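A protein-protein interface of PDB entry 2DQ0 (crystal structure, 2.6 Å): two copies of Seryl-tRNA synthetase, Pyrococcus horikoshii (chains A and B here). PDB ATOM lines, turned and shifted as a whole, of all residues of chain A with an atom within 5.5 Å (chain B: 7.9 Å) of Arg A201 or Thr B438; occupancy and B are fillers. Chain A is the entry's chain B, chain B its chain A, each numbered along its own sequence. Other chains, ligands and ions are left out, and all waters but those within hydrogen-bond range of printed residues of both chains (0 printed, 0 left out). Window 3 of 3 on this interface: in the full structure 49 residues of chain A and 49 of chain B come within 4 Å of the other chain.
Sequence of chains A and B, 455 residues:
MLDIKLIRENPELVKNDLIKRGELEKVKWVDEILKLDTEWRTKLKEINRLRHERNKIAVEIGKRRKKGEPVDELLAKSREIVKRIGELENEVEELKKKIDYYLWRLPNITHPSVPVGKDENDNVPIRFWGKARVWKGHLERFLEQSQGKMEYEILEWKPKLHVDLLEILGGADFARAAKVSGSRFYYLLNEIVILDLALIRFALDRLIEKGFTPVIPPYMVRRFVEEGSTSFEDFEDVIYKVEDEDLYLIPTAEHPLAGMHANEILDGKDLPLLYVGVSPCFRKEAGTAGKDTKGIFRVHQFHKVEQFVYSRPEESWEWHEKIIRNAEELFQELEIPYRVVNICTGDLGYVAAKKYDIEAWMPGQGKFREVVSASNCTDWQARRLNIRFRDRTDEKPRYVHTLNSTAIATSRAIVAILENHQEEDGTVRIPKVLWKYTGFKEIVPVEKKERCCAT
NH2 of Arg B201 is in hydrogen-bond range of O of Tyr A437 (3.0 Å). The backbone carbonyl oxygen of Tyr B437 is in hydrogen-bond range of the guanidinium group of Arg A201, at 2.8 Å.
Of the printed residues of chain B, Leu A197 touches Arg B201. Of the printed residues of chain B, Ile A200 touches Leu B197. Of the printed residues of chain B, Arg A201 touches Leu B197, Tyr B437 and Thr B438. Printed residues of chain B within 4 Å of Leu A204: Leu B197 (3.6 Å). Of the printed residues of chain A, Arg B201 touches Leu A197 (3.7 Å) and Tyr A437 (3.0 Å). Val B433 touches none of the printed residues of chain A. Of the printed residues of chain A, Tyr B437 touches Arg A201 (2.8 Å). Of the printed residues of chain A, Thr B438 touches Arg A201 (3.99 Å). Phe B440 touches none of the printed residues of chain A. The nearest printed residue of chain B that does not touch Leu A204 is Val B193 (4.7 Å).
Of the 12 printed residues of chain A, 5 touch a printed residue of chain B. Printed residues of chain B that touch a printed residue of chain A: Leu B197, Arg B201, Tyr B437 and Thr B438. Hydrophobic or aromatic side chains of chain B within 4 Å of the printed part of chain A: Leu B197.
Leu A197 touches Arg B201, and with the chains exchanged Arg A201 touches Leu B197. Arg A201 touches Tyr B437, and with the chains exchanged Tyr A437 touches Arg B201. Of the 7 pairs that touch across the chains among the printed residues, 4 have their exchanged pair printed and touching as well.
The side-chain hydroxyl (OH) of Tyr A437 lies within hydrogen-bond range of the side-chain carboxylate (OD2) of Asp A205 (2.5 Å). The side-chain carboxylate of Asp A205 is in salt-bridge range of the guanidinium group of Arg A201. The side-chain hydroxyl (OG1) of Thr B438 is in hydrogen-bond range of the backbone carbonyl oxygen (O) of Phe B440 (2.8 Å). OG1 of Thr B438 sits at hydrogen-bond distance from O of Leu B434.
Among the printed residues, pairs that only touch across the chains: Leu A197 with Arg B201 (3.7 Å), Ile A200 with Leu B197 (3.8 Å), Arg A201 with Leu B197 (3.7 Å), Arg A201 with Thr B438 (3.99 Å) and Leu A204 with Leu B197 (3.6 Å).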
ATOM      1  N   ASP A 196     -15.756   8.488  38.635  1.00  0.00           N
ATOM      2  CA  ASP A 196     -16.592   7.412  38.143  1.00  0.00           C
ATOM      3  C   ASP A 196     -17.192   7.770  36.774  1.00  0.00           C
ATOM      4  O   ASP A 196     -17.018   7.032  35.794  1.00  0.00           O
ATOM      5  CB  ASP A 196     -17.704   7.117  39.153  1.00  0.00           C
ATOM      6  CG  ASP A 196     -18.581   5.948  38.732  1.00  0.00           C
ATOM      7  OD1 ASP A 196     -19.242   6.035  37.683  1.00  0.00           O
ATOM      8  OD2 ASP A 196     -18.613   4.937  39.447  1.00  0.00           O
ATOM      9  N   LEU A 197     -17.892   8.897  36.695  1.00  0.00           N
ATOM     10  CA  LEU A 197     -18.475   9.299  35.421  1.00  0.00           C
ATOM     11  C   LEU A 197     -17.390   9.539  34.356  1.00  0.00           C
ATOM     12  O   LEU A 197     -17.569   9.177  33.195  1.00  0.00           O
ATOM     13  CB  LEU A 197     -19.318  10.560  35.595  1.00  0.00           C
ATOM     14  CG  LEU A 197     -20.425  10.508  36.660  1.00  0.00           C
ATOM     15  CD1 LEU A 197     -21.157  11.824  36.592  1.00  0.00           C
ATOM     16  CD2 LEU A 197     -21.425   9.363  36.436  1.00  0.00           C
ATOM     17  N   ALA A 198     -16.269  10.137  34.755  1.00  0.00           N
ATOM     18  CA  ALA A 198     -15.170  10.409  33.839  1.00  0.00           C
ATOM     19  C   ALA A 198     -14.636   9.135  33.199  1.00  0.00           C
ATOM     20  O   ALA A 198     -14.243   9.139  32.018  1.00  0.00           O
ATOM     21  CB  ALA A 198     -14.046  11.143  34.556  1.00  0.00           C
ATOM     22  N   LEU A 199     -14.615   8.047  33.967  1.00  0.00           N
ATOM     23  CA  LEU A 199     -14.148   6.768  33.437  1.00  0.00           C
ATOM     24  C   LEU A 199     -15.154   6.245  32.389  1.00  0.00           C
ATOM     25  O   LEU A 199     -14.769   5.721  31.346  1.00  0.00           O
ATOM     26  CB  LEU A 199     -13.938   5.746  34.572  1.00  0.00           C
ATOM     27  CG  LEU A 199     -12.730   5.965  35.497  1.00  0.00           C
ATOM     28  CD1 LEU A 199     -12.851   5.101  36.749  1.00  0.00           C
ATOM     29  CD2 LEU A 199     -11.458   5.635  34.738  1.00  0.00           C
ATOM     30  N   ILE A 200     -16.442   6.400  32.653  1.00  0.00           N
ATOM     31  CA  ILE A 200     -17.423   5.966  31.684  1.00  0.00           C
ATOM     32  C   ILE A 200     -17.244   6.752  30.376  1.00  0.00           C
ATOM     33  O   ILE A 200     -17.218   6.150  29.295  1.00  0.00           O
ATOM     34  CB  ILE A 200     -18.853   6.175  32.217  1.00  0.00           C
ATOM     35  CG1 ILE A 200     -19.156   5.117  33.282  1.00  0.00           C
ATOM     36  CG2 ILE A 200     -19.872   6.120  31.064  1.00  0.00           C
ATOM     37  CD1 ILE A 200     -20.343   5.472  34.164  1.00  0.00           C
ATOM     38  N   ARG A 201     -17.114   8.084  30.465  1.00  0.00           N
ATOM     39  CA  ARG A 201     -16.957   8.889  29.244  1.00  0.00           C
ATOM     40  C   ARG A 201     -15.667   8.583  28.517  1.00  0.00           C
ATOM     41  O   ARG A 201     -15.633   8.542  27.291  1.00  0.00           O
ATOM     42  CB  ARG A 201     -17.055  10.401  29.507  1.00  0.00           C
ATOM     43  CG  ARG A 201     -18.416  10.984  29.143  1.00  0.00           C
ATOM     44  CD  ARG A 201     -18.887  10.552  27.728  1.00  0.00           C
ATOM     45  NE  ARG A 201     -18.372  11.353  26.613  1.00  0.00           N
ATOM     46  CZ  ARG A 201     -18.640  12.648  26.447  1.00  0.00           C
ATOM     47  NH1 ARG A 201     -18.141  13.309  25.401  1.00  0.00           N
ATOM     48  NH2 ARG A 201     -19.396  13.290  27.344  1.00  0.00           N
ATOM     49  N   PHE A 202     -14.605   8.358  29.276  1.00  0.00           N
ATOM     50  CA  PHE A 202     -13.329   8.029  28.671  1.00  0.00           C
ATOM     51  C   PHE A 202     -13.463   6.725  27.877  1.00  0.00           C
ATOM     52  O   PHE A 202     -13.097   6.687  26.706  1.00  0.00           O
ATOM     53  CB  PHE A 202     -12.260   7.935  29.756  1.00  0.00           C
ATOM     54  CG  PHE A 202     -10.998   7.299  29.310  1.00  0.00           C
ATOM     55  CD1 PHE A 202     -10.323   7.772  28.206  1.00  0.00           C
ATOM     56  CD2 PHE A 202     -10.477   6.207  30.008  1.00  0.00           C
ATOM     57  CE1 PHE A 202      -9.146   7.177  27.793  1.00  0.00           C
ATOM     58  CE2 PHE A 202      -9.300   5.598  29.608  1.00  0.00           C
ATOM     59  CZ  PHE A 202      -8.627   6.080  28.497  1.00  0.00           C
ATOM     60  N   ALA A 203     -14.021   5.675  28.486  1.00  0.00           N
ATOM     61  CA  ALA A 203     -14.193   4.390  27.786  1.00  0.00           C
ATOM     62  C   ALA A 203     -15.086   4.511  26.546  1.00  0.00           C
ATOM     63  O   ALA A 203     -14.782   3.943  25.489  1.00  0.00           O
ATOM     64  CB  ALA A 203     -14.750   3.328  28.732  1.00  0.00           C
ATOM     65  N   LEU A 204     -16.190   5.237  26.674  1.00  0.00           N
ATOM     66  CA  LEU A 204     -17.077   5.454  25.536  1.00  0.00           C
ATOM     67  C   LEU A 204     -16.359   6.171  24.384  1.00  0.00           C
ATOM     68  O   LEU A 204     -16.371   5.686  23.254  1.00  0.00           O
ATOM     69  CB  LEU A 204     -18.288   6.275  25.962  1.00  0.00           C
ATOM     70  CG  LEU A 204     -19.681   5.643  26.044  1.00  0.00           C
ATOM     71  CD1 LEU A 204     -19.647   4.122  26.155  1.00  0.00           C
ATOM     72  CD2 LEU A 204     -20.361   6.244  27.254  1.00  0.00           C
ATOM     73  N   ASP A 205     -15.724   7.311  24.655  1.00  0.00           N
ATOM     74  CA  ASP A 205     -15.040   8.040  23.578  1.00  0.00           C
ATOM     75  C   ASP A 205     -14.047   7.117  22.870  1.00  0.00           C
ATOM     76  O   ASP A 205     -13.950   7.101  21.637  1.00  0.00           O
ATOM     77  CB  ASP A 205     -14.283   9.291  24.094  1.00  0.00           C
ATOM     78  CG  ASP A 205     -15.215  10.404  24.614  1.00  0.00           C
ATOM     79  OD1 ASP A 205     -16.433  10.368  24.344  1.00  0.00           O
ATOM     80  OD2 ASP A 205     -14.717  11.335  25.293  1.00  0.00           O
ATOM     81  N   ARG A 206     -13.315   6.320  23.626  1.00  0.00           N
ATOM     82  CA  ARG A 206     -12.357   5.463  22.956  1.00  0.00           C
ATOM     83  C   ARG A 206     -13.013   4.415  22.095  1.00  0.00           C
ATOM     84  O   ARG A 206     -12.589   4.207  20.970  1.00  0.00           O
ATOM     85  CB  ARG A 206     -11.401   4.807  23.947  1.00  0.00           C
ATOM     86  CG  ARG A 206      -9.943   5.097  23.622  1.00  0.00           C
ATOM     87  CD  ARG A 206      -9.676   6.596  23.575  1.00  0.00           C
ATOM     88  NE  ARG A 206      -8.279   6.897  23.869  1.00  0.00           N
ATOM     89  CZ  ARG A 206      -7.836   8.096  24.253  1.00  0.00           C
ATOM     90  NH1 ARG A 206      -8.668   9.134  24.389  1.00  0.00           N
ATOM     91  NH2 ARG A 206      -6.553   8.255  24.532  1.00  0.00           N
ATOM     92  N   TYR A 437     -11.492  15.066  31.523  1.00  0.00           N
ATOM     93  CA  TYR A 437     -12.793  14.652  32.035  1.00  0.00           C
ATOM     94  C   TYR A 437     -13.072  15.048  33.475  1.00  0.00           C
ATOM     95  O   TYR A 437     -14.164  15.516  33.788  1.00  0.00           O
ATOM     96  CB  TYR A 437     -12.970  13.143  31.911  1.00  0.00           C
ATOM     97  CG  TYR A 437     -12.858  12.604  30.502  1.00  0.00           C
ATOM     98  CD1 TYR A 437     -11.679  12.018  30.044  1.00  0.00           C
ATOM     99  CD2 TYR A 437     -13.946  12.658  29.634  1.00  0.00           C
ATOM    100  CE1 TYR A 437     -11.593  11.493  28.748  1.00  0.00           C
ATOM    101  CE2 TYR A 437     -13.869  12.136  28.339  1.00  0.00           C
ATOM    102  CZ  TYR A 437     -12.699  11.560  27.909  1.00  0.00           C
ATOM    103  OH  TYR A 437     -12.639  11.059  26.641  1.00  0.00           O
ATOM    104  N   GLU B 191     -25.410   9.639  19.394  1.00  0.00           N
ATOM    105  CA  GLU B 191     -25.258  10.921  20.034  1.00  0.00           C
ATOM    106  C   GLU B 191     -26.226  11.142  21.180  1.00  0.00           C
ATOM    107  O   GLU B 191     -25.918  11.879  22.115  1.00  0.00           O
ATOM    108  CB  GLU B 191     -25.310  12.052  18.999  1.00  0.00           C
ATOM    109  CG  GLU B 191     -26.113  11.698  17.778  1.00  0.00           C
ATOM    110  CD  GLU B 191     -25.309  10.987  16.710  1.00  0.00           C
ATOM    111  OE1 GLU B 191     -25.772   9.932  16.239  1.00  0.00           O
ATOM    112  OE2 GLU B 191     -24.235  11.487  16.324  1.00  0.00           O
ATOM    113  N   VAL B 193     -26.864   9.063  23.457  1.00  0.00           N
ATOM    114  CA  VAL B 193     -26.239   8.503  24.651  1.00  0.00           C
ATOM    115  C   VAL B 193     -25.261   9.539  25.193  1.00  0.00           C
ATOM    116  O   VAL B 193     -25.189   9.764  26.405  1.00  0.00           O
ATOM    117  CB  VAL B 193     -25.484   7.178  24.350  1.00  0.00           C
ATOM    118  CG1 VAL B 193     -24.721   6.723  25.576  1.00  0.00           C
ATOM    119  CG2 VAL B 193     -26.474   6.091  23.946  1.00  0.00           C
ATOM    120  N   ILE B 194     -24.513  10.185  24.299  1.00  0.00           N
ATOM    121  CA  ILE B 194     -23.578  11.204  24.742  1.00  0.00           C
ATOM    122  C   ILE B 194     -24.344  12.378  25.343  1.00  0.00           C
ATOM    123  O   ILE B 194     -23.927  12.960  26.341  1.00  0.00           O
ATOM    124  CB  ILE B 194     -22.667  11.710  23.583  1.00  0.00           C
ATOM    125  CG1 ILE B 194     -21.339  10.947  23.563  1.00  0.00           C
ATOM    126  CG2 ILE B 194     -22.274  13.150  23.825  1.00  0.00           C
ATOM    127  CD1 ILE B 194     -21.464   9.473  23.615  1.00  0.00           C
ATOM    128  N   LEU B 195     -25.472  12.720  24.731  1.00  0.00           N
ATOM    129  CA  LEU B 195     -26.280  13.829  25.222  1.00  0.00           C
ATOM    130  C   LEU B 195     -26.800  13.574  26.650  1.00  0.00           C
ATOM    131  O   LEU B 195     -26.826  14.480  27.494  1.00  0.00           O
ATOM    132  CB  LEU B 195     -27.453  14.082  24.259  1.00  0.00           C
ATOM    133  CG  LEU B 195     -28.375  15.213  24.680  1.00  0.00           C
ATOM    134  CD1 LEU B 195     -27.579  16.511  24.785  1.00  0.00           C
ATOM    135  CD2 LEU B 195     -29.489  15.343  23.687  1.00  0.00           C
ATOM    136  N   ASP B 196     -27.217  12.332  26.898  1.00  0.00           N
ATOM    137  CA  ASP B 196     -27.733  11.914  28.186  1.00  0.00           C
ATOM    138  C   ASP B 196     -26.627  12.114  29.222  1.00  0.00           C
ATOM    139  O   ASP B 196     -26.836  12.816  30.223  1.00  0.00           O
ATOM    140  CB  ASP B 196     -28.149  10.439  28.123  1.00  0.00           C
ATOM    141  CG  ASP B 196     -28.792   9.938  29.416  1.00  0.00           C
ATOM    142  OD1 ASP B 196     -29.832   9.266  29.334  1.00  0.00           O
ATOM    143  OD2 ASP B 196     -28.265  10.185  30.515  1.00  0.00           O
ATOM    144  N   LEU B 197     -25.459  11.512  28.987  1.00  0.00           N
ATOM    145  CA  LEU B 197     -24.354  11.680  29.930  1.00  0.00           C
ATOM    146  C   LEU B 197     -23.962  13.136  30.107  1.00  0.00           C
ATOM    147  O   LEU B 197     -23.665  13.563  31.225  1.00  0.00           O
ATOM    148  CB  LEU B 197     -23.108  10.916  29.505  1.00  0.00           C
ATOM    149  CG  LEU B 197     -23.191   9.394  29.412  1.00  0.00           C
ATOM    150  CD1 LEU B 197     -21.755   8.884  29.346  1.00  0.00           C
ATOM    151  CD2 LEU B 197     -23.954   8.774  30.617  1.00  0.00           C
ATOM    152  N   ALA B 198     -23.959  13.884  29.009  1.00  0.00           N
ATOM    153  CA  ALA B 198     -23.596  15.295  29.047  1.00  0.00           C
ATOM    154  C   ALA B 198     -24.517  16.064  29.977  1.00  0.00           C
ATOM    155  O   ALA B 198     -24.048  16.880  30.779  1.00  0.00           O
ATOM    156  CB  ALA B 198     -23.642  15.893  27.641  1.00  0.00           C
ATOM    157  N   LEU B 199     -25.818  15.790  29.880  1.00  0.00           N
ATOM    158  CA  LEU B 199     -26.804  16.460  30.726  1.00  0.00           C
ATOM    159  C   LEU B 199     -26.562  16.196  32.222  1.00  0.00           C
ATOM    160  O   LEU B 199     -26.737  17.088  33.040  1.00  0.00           O
ATOM    161  CB  LEU B 199     -28.221  16.041  30.302  1.00  0.00           C
ATOM    162  CG  LEU B 199     -28.774  16.775  29.068  1.00  0.00           C
ATOM    163  CD1 LEU B 199     -30.059  16.121  28.517  1.00  0.00           C
ATOM    164  CD2 LEU B 199     -29.058  18.198  29.474  1.00  0.00           C
ATOM    165  N   ARG B 201     -23.520  15.425  33.690  1.00  0.00           N
ATOM    166  CA  ARG B 201     -22.337  16.198  34.055  1.00  0.00           C
ATOM    167  C   ARG B 201     -22.615  17.692  34.204  1.00  0.00           C
ATOM    168  O   ARG B 201     -22.172  18.315  35.167  1.00  0.00           O
ATOM    169  CB  ARG B 201     -21.209  16.007  33.034  1.00  0.00           C
ATOM    170  CG  ARG B 201     -20.294  14.819  33.313  1.00  0.00           C
ATOM    171  CD  ARG B 201     -19.851  14.737  34.786  1.00  0.00           C
ATOM    172  NE  ARG B 201     -19.025  15.850  35.273  1.00  0.00           N
ATOM    173  CZ  ARG B 201     -17.701  15.930  35.132  1.00  0.00           C
ATOM    174  NH1 ARG B 201     -17.049  16.977  35.622  1.00  0.00           N
ATOM    175  NH2 ARG B 201     -17.026  14.971  34.496  1.00  0.00           N
ATOM    176  N   ILE B 430     -27.713  21.559  19.423  1.00  0.00           N
ATOM    177  CA  ILE B 430     -27.588  21.379  20.854  1.00  0.00           C
ATOM    178  C   ILE B 430     -27.073  22.674  21.477  1.00  0.00           C
ATOM    179  O   ILE B 430     -26.166  23.298  20.960  1.00  0.00           O
ATOM    180  CB  ILE B 430     -26.717  20.099  21.214  1.00  0.00           C
ATOM    181  CG1 ILE B 430     -25.393  20.492  21.810  1.00  0.00           C
ATOM    182  CG2 ILE B 430     -26.533  19.201  20.014  1.00  0.00           C
ATOM    183  CD1 ILE B 430     -25.496  20.623  23.287  1.00  0.00           C
ATOM    184  N   PRO B 431     -27.697  23.112  22.582  1.00  0.00           N
ATOM    185  CA  PRO B 431     -27.350  24.337  23.321  1.00  0.00           C
ATOM    186  C   PRO B 431     -25.848  24.482  23.551  1.00  0.00           C
ATOM    187  O   PRO B 431     -25.200  23.545  24.012  1.00  0.00           O
ATOM    188  CB  PRO B 431     -28.096  24.174  24.643  1.00  0.00           C
ATOM    189  CG  PRO B 431     -29.267  23.305  24.284  1.00  0.00           C
ATOM    190  CD  PRO B 431     -28.699  22.310  23.312  1.00  0.00           C
ATOM    191  N   LYS B 432     -25.312  25.666  23.264  1.00  0.00           N
ATOM    192  CA  LYS B 432     -23.878  25.946  23.421  1.00  0.00           C
ATOM    193  C   LYS B 432     -23.289  25.499  24.776  1.00  0.00           C
ATOM    194  O   LYS B 432     -22.185  24.984  24.839  1.00  0.00           O
ATOM    195  CB  LYS B 432     -23.609  27.453  23.190  1.00  0.00           C
ATOM    196  CG  LYS B 432     -24.301  27.989  21.915  1.00  0.00           C
ATOM    197  CD  LYS B 432     -24.320  29.530  21.812  1.00  0.00           C
ATOM    198  CE  LYS B 432     -25.307  30.047  20.732  1.00  0.00           C
ATOM    199  NZ  LYS B 432     -24.894  29.777  19.324  1.00  0.00           N
ATOM    200  N   VAL B 433     -24.032  25.689  25.851  1.00  0.00           N
ATOM    201  CA  VAL B 433     -23.555  25.311  27.167  1.00  0.00           C
ATOM    202  C   VAL B 433     -23.120  23.852  27.251  1.00  0.00           C
ATOM    203  O   VAL B 433     -22.256  23.524  28.064  1.00  0.00           O
ATOM    204  CB  VAL B 433     -24.636  25.516  28.247  1.00  0.00           C
ATOM    205  CG1 VAL B 433     -23.983  25.595  29.619  1.00  0.00           C
ATOM    206  CG2 VAL B 433     -25.443  26.760  27.942  1.00  0.00           C
ATOM    207  N   LEU B 434     -23.718  22.981  26.435  1.00  0.00           N
ATOM    208  CA  LEU B 434     -23.370  21.555  26.466  1.00  0.00           C
ATOM    209  C   LEU B 434     -22.239  21.142  25.528  1.00  0.00           C
ATOM    210  O   LEU B 434     -21.719  20.029  25.642  1.00  0.00           O
ATOM    211  CB  LEU B 434     -24.602  20.677  26.172  1.00  0.00           C
ATOM    212  CG  LEU B 434     -25.814  20.821  27.095  1.00  0.00           C
ATOM    213  CD1 LEU B 434     -26.988  20.055  26.566  1.00  0.00           C
ATOM    214  CD2 LEU B 434     -25.445  20.349  28.485  1.00  0.00           C
ATOM    215  N   TRP B 435     -21.851  22.020  24.608  1.00  0.00           N
ATOM    216  CA  TRP B 435     -20.779  21.703  23.654  1.00  0.00           C
ATOM    217  C   TRP B 435     -19.492  21.169  24.312  1.00  0.00           C
ATOM    218  O   TRP B 435     -18.825  20.282  23.764  1.00  0.00           O
ATOM    219  CB  TRP B 435     -20.430  22.928  22.808  1.00  0.00           C
ATOM    220  CG  TRP B 435     -21.516  23.424  21.895  1.00  0.00           C
ATOM    221  CD1 TRP B 435     -22.746  22.867  21.691  1.00  0.00           C
ATOM    222  CD2 TRP B 435     -21.458  24.577  21.055  1.00  0.00           C
ATOM    223  NE1 TRP B 435     -23.458  23.601  20.775  1.00  0.00           N
ATOM    224  CE2 TRP B 435     -22.691  24.657  20.366  1.00  0.00           C
ATOM    225  CE3 TRP B 435     -20.484  25.554  20.817  1.00  0.00           C
ATOM    226  CZ2 TRP B 435     -22.974  25.676  19.454  1.00  0.00           C
ATOM    227  CZ3 TRP B 435     -20.764  26.567  19.914  1.00  0.00           C
ATOM    228  CH2 TRP B 435     -22.000  26.622  19.241  1.00  0.00           C
ATOM    229  N   LYS B 436     -19.131  21.706  25.476  1.00  0.00           N
ATOM    230  CA  LYS B 436     -17.929  21.240  26.140  1.00  0.00           C
ATOM    231  C   LYS B 436     -18.116  19.799  26.599  1.00  0.00           C
ATOM    232  O   LYS B 436     -17.144  19.046  26.717  1.00  0.00           O
ATOM    233  CB  LYS B 436     -17.546  22.146  27.322  1.00  0.00           C
ATOM    234  CG  LYS B 436     -18.582  22.294  28.431  1.00  0.00           C
ATOM    235  CD  LYS B 436     -18.076  23.312  29.459  1.00  0.00           C
ATOM    236  CE  LYS B 436     -19.135  23.741  30.481  1.00  0.00           C
ATOM    237  NZ  LYS B 436     -20.069  24.817  29.998  1.00  0.00           N
ATOM    238  N   TYR B 437     -19.366  19.393  26.812  1.00  0.00           N
ATOM    239  CA  TYR B 437     -19.629  18.027  27.264  1.00  0.00           C
ATOM    240  C   TYR B 437     -19.880  17.018  26.154  1.00  0.00           C
ATOM    241  O   TYR B 437     -19.492  15.854  26.282  1.00  0.00           O
ATOM    242  CB  TYR B 437     -20.824  17.994  28.210  1.00  0.00           C
ATOM    243  CG  TYR B 437     -20.676  18.844  29.439  1.00  0.00           C
ATOM    244  CD1 TYR B 437     -21.320  20.070  29.530  1.00  0.00           C
ATOM    245  CD2 TYR B 437     -19.918  18.408  30.530  1.00  0.00           C
ATOM    246  CE1 TYR B 437     -21.222  20.854  30.683  1.00  0.00           C
ATOM    247  CE2 TYR B 437     -19.816  19.186  31.696  1.00  0.00           C
ATOM    248  CZ  TYR B 437     -20.474  20.405  31.762  1.00  0.00           C
ATOM    249  OH  TYR B 437     -20.420  21.172  32.903  1.00  0.00           O
ATOM    250  N   THR B 438     -20.527  17.461  25.074  1.00  0.00           N
ATOM    251  CA  THR B 438     -20.862  16.575  23.956  1.00  0.00           C
ATOM    252  C   THR B 438     -19.832  16.441  22.848  1.00  0.00           C
ATOM    253  O   THR B 438     -19.628  15.352  22.313  1.00  0.00           O
ATOM    254  CB  THR B 438     -22.168  17.015  23.258  1.00  0.00           C
ATOM    255  OG1 THR B 438     -22.031  18.370  22.803  1.00  0.00           O
ATOM    256  CG2 THR B 438     -23.340  16.899  24.200  1.00  0.00           C
ATOM    257  N   GLY B 439     -19.215  17.557  22.485  1.00  0.00           N
ATOM    258  CA  GLY B 439     -18.260  17.550  21.403  1.00  0.00           C
ATOM    259  C   GLY B 439     -18.987  18.156  20.224  1.00  0.00           C
ATOM    260  O   GLY B 439     -18.717  19.287  19.818  1.00  0.00           O
ATOM    261  N   PHE B 440     -19.947  17.418  19.696  1.00  0.00           N
ATOM    262  CA  PHE B 440     -20.727  17.866  18.561  1.00  0.00           C
ATOM    263  C   PHE B 440     -21.644  19.036  18.928  1.00  0.00           C
ATOM    264  O   PHE B 440     -22.012  19.186  20.074  1.00  0.00           O
ATOM    265  CB  PHE B 440     -21.529  16.690  18.048  1.00  0.00           C
ATOM    266  CG  PHE B 440     -22.413  16.057  19.092  1.00  0.00           C
ATOM    267  CD1 PHE B 440     -23.693  16.557  19.340  1.00  0.00           C
ATOM    268  CD2 PHE B 440     -21.990  14.922  19.784  1.00  0.00           C
ATOM    269  CE1 PHE B 440     -24.534  15.920  20.260  1.00  0.00           C
ATOM    270  CE2 PHE B 440     -22.828  14.277  20.709  1.00  0.00           C
ATOM    271  CZ  PHE B 440     -24.098  14.769  20.950  1.00  0.00           C
ATOM    272  N   LYS B 441     -22.014  19.862  17.950  1.00  0.00           N
ATOM    273  CA  LYS B 441     -22.880  21.017  18.219  1.00  0.00           C
ATOM    274  C   LYS B 441     -24.315  20.796  17.761  1.00  0.00           C
ATOM    275  O   LYS B 441     -25.224  21.533  18.138  1.00  0.00           O
ATOM    276  CB  LYS B 441     -22.327  22.268  17.542  1.00  0.00           C
ATOM    277  CG  LYS B 441     -20.943  22.695  18.030  1.00  0.00           C
ATOM    278  CD  LYS B 441     -20.533  24.014  17.408  1.00  0.00           C
ATOM    279  CE  LYS B 441     -19.107  24.368  17.768  1.00  0.00           C
ATOM    280  NZ  LYS B 441     -18.165  23.295  17.364  1.00  0.00           N
ATOM    281  N   GLU B 442     -24.524  19.769  16.951  1.00  0.00           N
ATOM    282  CA  GLU B 442     -25.857  19.466  16.477  1.00  0.00           C
ATOM    283  C   GLU B 442     -25.928  17.986  16.141  1.00  0.00           C
ATOM    284  O   GLU B 442     -24.907  17.295  16.102  1.00  0.00           O
ATOM    285  CB  GLU B 442     -26.164  20.281  15.224  1.00  0.00           C
ATOM    286  CG  GLU B 442     -25.080  20.181  14.148  1.00  0.00           C
ATOM    287  CD  GLU B 442     -25.483  20.846  12.837  1.00  0.00           C
ATOM    288  OE1 GLU B 442     -26.015  21.988  12.877  1.00  0.00           O
ATOM    289  OE2 GLU B 442     -25.255  20.228  11.767  1.00  0.00           O
ATOM    290  N   ILE B 443     -27.137  17.490  15.918  1.00  0.00           N
ATOM    291  CA  ILE B 443     -27.296  16.099  15.545  1.00  0.00           C
ATOM    292  C   ILE B 443     -28.062  16.103  14.240  1.00  0.00           C
ATOM    293  O   ILE B 443     -29.170  16.619  14.171  1.00  0.00           O
ATOM    294  CB  ILE B 443     -28.069  15.278  16.610  1.00  0.00           C
ATOM    295  CG1 ILE B 443     -27.392  15.434  17.983  1.00  0.00           C
ATOM    296  CG2 ILE B 443     -28.090  13.801  16.182  1.00  0.00           C
ATOM    297  CD1 ILE B 443     -28.172  14.869  19.136  1.00  0.00           C
